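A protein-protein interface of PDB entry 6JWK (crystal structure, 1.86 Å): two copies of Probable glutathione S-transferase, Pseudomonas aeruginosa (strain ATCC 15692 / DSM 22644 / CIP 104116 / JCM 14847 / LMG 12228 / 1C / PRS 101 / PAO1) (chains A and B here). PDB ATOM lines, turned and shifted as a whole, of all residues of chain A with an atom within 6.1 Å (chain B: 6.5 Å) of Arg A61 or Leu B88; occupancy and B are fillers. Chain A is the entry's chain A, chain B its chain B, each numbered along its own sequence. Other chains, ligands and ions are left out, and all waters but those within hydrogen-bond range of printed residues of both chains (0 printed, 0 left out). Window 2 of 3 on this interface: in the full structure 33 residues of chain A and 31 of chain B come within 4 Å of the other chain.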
ATOM      1  N   LEU A  55     -14.553 -14.988 -28.713  1.00  0.00           N
ATOM      2  CA  LEU A  55     -14.716 -14.843 -27.255  1.00  0.00           C
ATOM      3  C   LEU A  55     -13.506 -15.517 -26.579  1.00  0.00           C
ATOM      4  O   LEU A  55     -13.208 -16.714 -26.887  1.00  0.00           O
ATOM      5  CB  LEU A  55     -16.030 -15.458 -26.776  1.00  0.00           C
ATOM      6  CG  LEU A  55     -16.326 -15.169 -25.312  1.00  0.00           C
ATOM      7  CD1 LEU A  55     -16.935 -13.786 -25.173  1.00  0.00           C
ATOM      8  CD2 LEU A  55     -17.233 -16.214 -24.695  1.00  0.00           C
ATOM      9  N   VAL A  56     -12.810 -14.760 -25.719  1.00  0.00           N
ATOM     10  CA  VAL A  56     -11.710 -15.257 -24.852  1.00  0.00           C
ATOM     11  C   VAL A  56     -12.267 -15.292 -23.436  1.00  0.00           C
ATOM     12  O   VAL A  56     -12.701 -14.230 -22.956  1.00  0.00           O
ATOM     13  CB  VAL A  56     -10.431 -14.414 -24.999  1.00  0.00           C
ATOM     14  CG1 VAL A  56      -9.296 -14.992 -24.171  1.00  0.00           C
ATOM     15  CG2 VAL A  56     -10.000 -14.288 -26.450  1.00  0.00           C
ATOM     16  N   ASP A  57     -12.363 -16.473 -22.819  1.00  0.00           N
ATOM     17  CA  ASP A  57     -12.944 -16.559 -21.453  1.00  0.00           C
ATOM     18  C   ASP A  57     -11.846 -16.302 -20.421  1.00  0.00           C
ATOM     19  O   ASP A  57     -10.717 -15.999 -20.838  1.00  0.00           O
ATOM     20  CB  ASP A  57     -13.673 -17.870 -21.196  1.00  0.00           C
ATOM     21  CG  ASP A  57     -12.796 -19.113 -21.132  1.00  0.00           C
ATOM     22  OD1 ASP A  57     -11.554 -18.984 -21.028  1.00  0.00           O
ATOM     23  OD2 ASP A  57     -13.379 -20.202 -21.213  1.00  0.00           O
ATOM     24  N   ALA A  58     -12.179 -16.442 -19.132  1.00  0.00           N
ATOM     25  CA  ALA A  58     -11.308 -16.120 -17.973  1.00  0.00           C
ATOM     26  C   ALA A  58     -10.057 -17.014 -17.944  1.00  0.00           C
ATOM     27  O   ALA A  58      -9.149 -16.683 -17.178  1.00  0.00           O
ATOM     28  CB  ALA A  58     -12.084 -16.254 -16.678  1.00  0.00           C
ATOM     29  N   ASP A  59     -10.011 -18.097 -18.729  1.00  0.00           N
ATOM     30  CA  ASP A  59      -8.897 -19.082 -18.736  1.00  0.00           C
ATOM     31  C   ASP A  59      -8.051 -18.897 -19.994  1.00  0.00           C
ATOM     32  O   ASP A  59      -7.094 -19.676 -20.180  1.00  0.00           O
ATOM     33  CB  ASP A  59      -9.463 -20.499 -18.619  1.00  0.00           C
ATOM     34  CG  ASP A  59     -10.165 -20.711 -17.288  1.00  0.00           C
ATOM     35  OD1 ASP A  59      -9.566 -20.355 -16.260  1.00  0.00           O
ATOM     36  OD2 ASP A  59     -11.289 -21.224 -17.281  1.00  0.00           O
ATOM     37  N   GLY A  60      -8.382 -17.917 -20.841  1.00  0.00           N
ATOM     38  CA  GLY A  60      -7.654 -17.703 -22.101  1.00  0.00           C
ATOM     39  C   GLY A  60      -8.108 -18.668 -23.179  1.00  0.00           C
ATOM     40  O   GLY A  60      -7.422 -18.735 -24.206  1.00  0.00           O
ATOM     41  N   ARG A  61      -9.208 -19.407 -22.985  1.00  0.00           N
ATOM     42  CA  ARG A  61      -9.730 -20.260 -24.101  1.00  0.00           C
ATOM     43  C   ARG A  61     -10.446 -19.360 -25.112  1.00  0.00           C
ATOM     44  O   ARG A  61     -11.084 -18.374 -24.690  1.00  0.00           O
ATOM     45  CB  ARG A  61     -10.597 -21.388 -23.551  1.00  0.00           C
ATOM     46  CG  ARG A  61      -9.774 -22.409 -22.792  1.00  0.00           C
ATOM     47  CD  ARG A  61     -10.608 -23.577 -22.361  1.00  0.00           C
ATOM     48  NE  ARG A  61      -9.769 -24.657 -21.861  1.00  0.00           N
ATOM     49  CZ  ARG A  61      -9.613 -24.941 -20.587  1.00  0.00           C
ATOM     50  NH1 ARG A  61     -10.162 -24.188 -19.644  1.00  0.00           N
ATOM     51  NH2 ARG A  61      -8.879 -25.979 -20.258  1.00  0.00           N
ATOM     52  N   ARG A  62     -10.238 -19.631 -26.400  1.00  0.00           N
ATOM     53  CA  ARG A  62     -10.786 -18.877 -27.557  1.00  0.00           C
ATOM     54  C   ARG A  62     -11.922 -19.680 -28.217  1.00  0.00           C
ATOM     55  O   ARG A  62     -11.726 -20.881 -28.447  1.00  0.00           O
ATOM     56  CB  ARG A  62      -9.674 -18.703 -28.582  1.00  0.00           C
ATOM     57  CG  ARG A  62      -8.430 -18.047 -28.011  1.00  0.00           C
ATOM     58  CD  ARG A  62      -7.373 -18.074 -29.076  1.00  0.00           C
ATOM     59  NE  ARG A  62      -6.234 -17.262 -28.744  1.00  0.00           N
ATOM     60  CZ  ARG A  62      -5.219 -17.073 -29.565  1.00  0.00           C
ATOM     61  NH1 ARG A  62      -4.197 -16.320 -29.193  1.00  0.00           N
ATOM     62  NH2 ARG A  62      -5.221 -17.648 -30.753  1.00  0.00           N
ATOM     63  N   PHE A  63     -13.043 -19.044 -28.565  1.00  0.00           N
ATOM     64  CA  PHE A  63     -14.189 -19.672 -29.279  1.00  0.00           C
ATOM     65  C   PHE A  63     -14.602 -18.747 -30.409  1.00  0.00           C
ATOM     66  O   PHE A  63     -14.651 -17.522 -30.087  1.00  0.00           O
ATOM     67  CB  PHE A  63     -15.334 -19.849 -28.296  1.00  0.00           C
ATOM     68  CG  PHE A  63     -15.011 -20.685 -27.093  1.00  0.00           C
ATOM     69  CD1 PHE A  63     -14.899 -22.065 -27.215  1.00  0.00           C
ATOM     70  CD2 PHE A  63     -14.840 -20.112 -25.847  1.00  0.00           C
ATOM     71  CE1 PHE A  63     -14.620 -22.852 -26.108  1.00  0.00           C
ATOM     72  CE2 PHE A  63     -14.565 -20.898 -24.734  1.00  0.00           C
ATOM     73  CZ  PHE A  63     -14.457 -22.265 -24.867  1.00  0.00           C
ATOM     74  N   TYR A  72     -22.457 -22.065 -24.964  1.00  0.00           N
ATOM     75  CA  TYR A  72     -21.491 -21.929 -23.844  1.00  0.00           C
ATOM     76  C   TYR A  72     -21.960 -20.868 -22.831  1.00  0.00           C
ATOM     77  O   TYR A  72     -21.981 -21.127 -21.637  1.00  0.00           O
ATOM     78  CB  TYR A  72     -20.154 -21.517 -24.409  1.00  0.00           C
ATOM     79  CG  TYR A  72     -19.041 -21.501 -23.402  1.00  0.00           C
ATOM     80  CD1 TYR A  72     -18.725 -22.640 -22.670  1.00  0.00           C
ATOM     81  CD2 TYR A  72     -18.268 -20.358 -23.228  1.00  0.00           C
ATOM     82  CE1 TYR A  72     -17.666 -22.631 -21.773  1.00  0.00           C
ATOM     83  CE2 TYR A  72     -17.212 -20.333 -22.336  1.00  0.00           C
ATOM     84  CZ  TYR A  72     -16.918 -21.477 -21.613  1.00  0.00           C
ATOM     85  OH  TYR A  72     -15.882 -21.436 -20.742  1.00  0.00           O
ATOM     86  N   LEU B  85     -21.877 -33.630 -22.611  1.00  0.00           N
ATOM     87  CA  LEU B  85     -22.591 -33.033 -21.460  1.00  0.00           C
ATOM     88  C   LEU B  85     -21.731 -31.926 -20.859  1.00  0.00           C
ATOM     89  O   LEU B  85     -22.281 -30.879 -20.495  1.00  0.00           O
ATOM     90  CB  LEU B  85     -22.849 -34.135 -20.425  1.00  0.00           C
ATOM     91  CG  LEU B  85     -24.155 -34.890 -20.614  1.00  0.00           C
ATOM     92  CD1 LEU B  85     -24.376 -35.865 -19.455  1.00  0.00           C
ATOM     93  CD2 LEU B  85     -25.306 -33.914 -20.743  1.00  0.00           C
ATOM     94  N   ASP B  86     -20.428 -32.151 -20.736  1.00  0.00           N
ATOM     95  CA  ASP B  86     -19.511 -31.128 -20.173  1.00  0.00           C
ATOM     96  C   ASP B  86     -19.538 -29.865 -21.046  1.00  0.00           C
ATOM     97  O   ASP B  86     -19.345 -29.959 -22.265  1.00  0.00           O
ATOM     98  CB  ASP B  86     -18.098 -31.659 -20.101  1.00  0.00           C
ATOM     99  CG  ASP B  86     -17.127 -30.639 -19.534  1.00  0.00           C
ATOM    100  OD1 ASP B  86     -16.853 -30.733 -18.352  1.00  0.00           O
ATOM    101  OD2 ASP B  86     -16.612 -29.802 -20.289  1.00  0.00           O
ATOM    102  N   PRO B  87     -19.708 -28.664 -20.447  1.00  0.00           N
ATOM    103  CA  PRO B  87     -19.928 -27.424 -21.196  1.00  0.00           C
ATOM    104  C   PRO B  87     -18.767 -26.972 -22.068  1.00  0.00           C
ATOM    105  O   PRO B  87     -18.965 -26.607 -23.215  1.00  0.00           O
ATOM    106  CB  PRO B  87     -20.119 -26.346 -20.111  1.00  0.00           C
ATOM    107  CG  PRO B  87     -20.631 -27.121 -18.933  1.00  0.00           C
ATOM    108  CD  PRO B  87     -19.932 -28.453 -18.999  1.00  0.00           C
ATOM    109  N   LEU B  88     -17.568 -27.073 -21.515  1.00  0.00           N
ATOM    110  CA  LEU B  88     -16.354 -26.785 -22.284  1.00  0.00           C
ATOM    111  C   LEU B  88     -16.218 -27.782 -23.460  1.00  0.00           C
ATOM    112  O   LEU B  88     -15.971 -27.320 -24.605  1.00  0.00           O
ATOM    113  CB  LEU B  88     -15.138 -26.821 -21.365  1.00  0.00           C
ATOM    114  CG  LEU B  88     -13.837 -26.651 -22.133  1.00  0.00           C
ATOM    115  CD1 LEU B  88     -13.854 -25.325 -22.847  1.00  0.00           C
ATOM    116  CD2 LEU B  88     -12.621 -26.763 -21.237  1.00  0.00           C
ATOM    117  N   HIS B  89     -16.364 -29.078 -23.217  1.00  0.00           N
ATOM    118  CA  HIS B  89     -16.176 -30.116 -24.256  1.00  0.00           C
ATOM    119  C   HIS B  89     -17.272 -29.895 -25.300  1.00  0.00           C
ATOM    120  O   HIS B  89     -17.004 -30.097 -26.492  1.00  0.00           O
ATOM    121  CB  HIS B  89     -16.183 -31.521 -23.623  1.00  0.00           C
ATOM    122  CG  HIS B  89     -15.085 -31.697 -22.622  1.00  0.00           C
ATOM    123  ND1 HIS B  89     -15.002 -32.801 -21.810  1.00  0.00           N
ATOM    124  CD2 HIS B  89     -14.030 -30.911 -22.301  1.00  0.00           C
ATOM    125  CE1 HIS B  89     -13.961 -32.676 -21.000  1.00  0.00           C
ATOM    126  NE2 HIS B  89     -13.328 -31.552 -21.313  1.00  0.00           N
ATOM    127  N   ARG B  90     -18.474 -29.512 -24.866  1.00  0.00           N
ATOM    128  CA  ARG B  90     -19.594 -29.268 -25.813  1.00  0.00           C
ATOM    129  C   ARG B  90     -19.242 -28.065 -26.713  1.00  0.00           C
ATOM    130  O   ARG B  90     -19.369 -28.183 -27.972  1.00  0.00           O
ATOM    131  CB  ARG B  90     -20.915 -29.071 -25.065  1.00  0.00           C
ATOM    132  CG  ARG B  90     -22.077 -28.830 -26.031  1.00  0.00           C
ATOM    133  CD  ARG B  90     -23.455 -28.907 -25.441  1.00  0.00           C
ATOM    134  NE  ARG B  90     -23.584 -27.997 -24.336  1.00  0.00           N
ATOM    135  CZ  ARG B  90     -23.445 -28.318 -23.055  1.00  0.00           C
ATOM    136  NH1 ARG B  90     -23.614 -27.387 -22.130  1.00  0.00           N
ATOM    137  NH2 ARG B  90     -23.148 -29.557 -22.687  1.00  0.00           N
ATOM    138  N   ALA B  91     -18.767 -26.953 -26.131  1.00  0.00           N
ATOM    139  CA  ALA B  91     -18.425 -25.724 -26.886  1.00  0.00           C
ATOM    140  C   ALA B  91     -17.368 -26.061 -27.933  1.00  0.00           C
ATOM    141  O   ALA B  91     -17.489 -25.620 -29.067  1.00  0.00           O
ATOM    142  CB  ALA B  91     -17.969 -24.609 -25.975  1.00  0.00           C
ATOM    143  N   GLN B  92     -16.380 -26.891 -27.567  1.00  0.00           N
ATOM    144  CA  GLN B  92     -15.289 -27.294 -28.484  1.00  0.00           C
ATOM    145  C   GLN B  92     -15.826 -28.192 -29.606  1.00  0.00           C
ATOM    146  O   GLN B  92     -15.428 -28.010 -30.741  1.00  0.00           O
ATOM    147  CB  GLN B  92     -14.199 -27.952 -27.630  1.00  0.00           C
ATOM    148  CG  GLN B  92     -13.420 -26.908 -26.844  1.00  0.00           C
ATOM    149  CD  GLN B  92     -12.357 -27.509 -25.950  1.00  0.00           C
ATOM    150  OE1 GLN B  92     -12.463 -28.651 -25.500  1.00  0.00           O
ATOM    151  NE2 GLN B  92     -11.379 -26.683 -25.604  1.00  0.00           N
ATOM    152  N   ALA B  93     -16.674 -29.159 -29.289  1.00  0.00           N
ATOM    153  CA  ALA B  93     -17.257 -30.068 -30.312  1.00  0.00           C
ATOM    154  C   ALA B  93     -18.159 -29.239 -31.246  1.00  0.00           C
ATOM    155  O   ALA B  93     -18.029 -29.359 -32.476  1.00  0.00           O
ATOM    156  CB  ALA B  93     -17.974 -31.174 -29.587  1.00  0.00           C
ATOM    157  N   ARG B 151     -10.558 -34.916 -27.414  1.00  0.00           N
ATOM    158  CA  ARG B 151     -10.475 -35.548 -26.078  1.00  0.00           C
ATOM    159  C   ARG B 151      -9.912 -36.963 -26.186  1.00  0.00           C
ATOM    160  O   ARG B 151      -9.559 -37.517 -25.149  1.00  0.00           O
ATOM    161  CB  ARG B 151     -11.835 -35.503 -25.390  1.00  0.00           C
ATOM    162  CG  ARG B 151     -12.336 -34.083 -25.151  1.00  0.00           C
ATOM    163  CD  ARG B 151     -11.570 -33.454 -23.991  1.00  0.00           C
ATOM    164  NE  ARG B 151     -11.412 -32.016 -24.120  1.00  0.00           N
ATOM    165  CZ  ARG B 151     -10.740 -31.267 -23.260  1.00  0.00           C
ATOM    166  NH1 ARG B 151     -10.162 -31.859 -22.218  1.00  0.00           N
ATOM    167  NH2 ARG B 151     -10.619 -29.955 -23.476  1.00  0.00           N
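No position is printed for both chains.
Printed residues of chain B that touch a printed residue of chain A: Leu B88 and Ala B91. Hydrophobic or aromatic side chains of chain B that line the printed part of chain A: Leu B88 and Ala B91. Hydrophobic or aromatic side chains of chain A that line the printed part of chain B: Phe A63 and Tyr A72. Along chain A the printed residues that touch a printed residue of chain B span positions 61 to 72.
Arg A61 touches just one residue of chain B: Leu B88 (3.6 Å). Printed residues of chain A within 4 Å of Ala B91: Phe A63 (3.8 Å) and Tyr A72 (3.9 Å). Of the printed residues of chain B, Phe A63 touches Leu B88 and Ala B91. Of the printed residues of chain B, Tyr A72 touches Ala B91. Val A56 touches none of the printed residues of chain B. His B89 touches none of the printed residues of chain A. The nearest residue of chain B that does not touch Arg A61 is Gln B92 (4.6 Å).
CD2 of Leu B88 touches CZ of Arg A61, 3.6 Å away. CD1 of Leu B88 touches CZ of Phe A63 (3.7 Å). CE1 of Phe A63 touches CB of Ala B91, at 3.8 Å. Tyr A72 touches Ala B91.
The side-chain carboxylate (OD2) of Asp B86 sits at hydrogen-bond distance from the backbone NH (N) of Leu B88, at 3.1 Å. NH1 of Arg A61 lies within salt-bridge range of OD2 of Asp A59. The backbone carbonyl oxygen (O) of Leu A55 sits at hydrogen-bond distance from the backbone NH (N) of Phe A63. The side-chain carboxylate of Asp A57 lies within hydrogen-bond range of the side-chain hydroxyl of Tyr A72 (2.8 Å). The side-chain carboxylate of Asp A57 sits at hydrogen-bond distance from the backbone NH of Arg A61 (3.1 Å).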
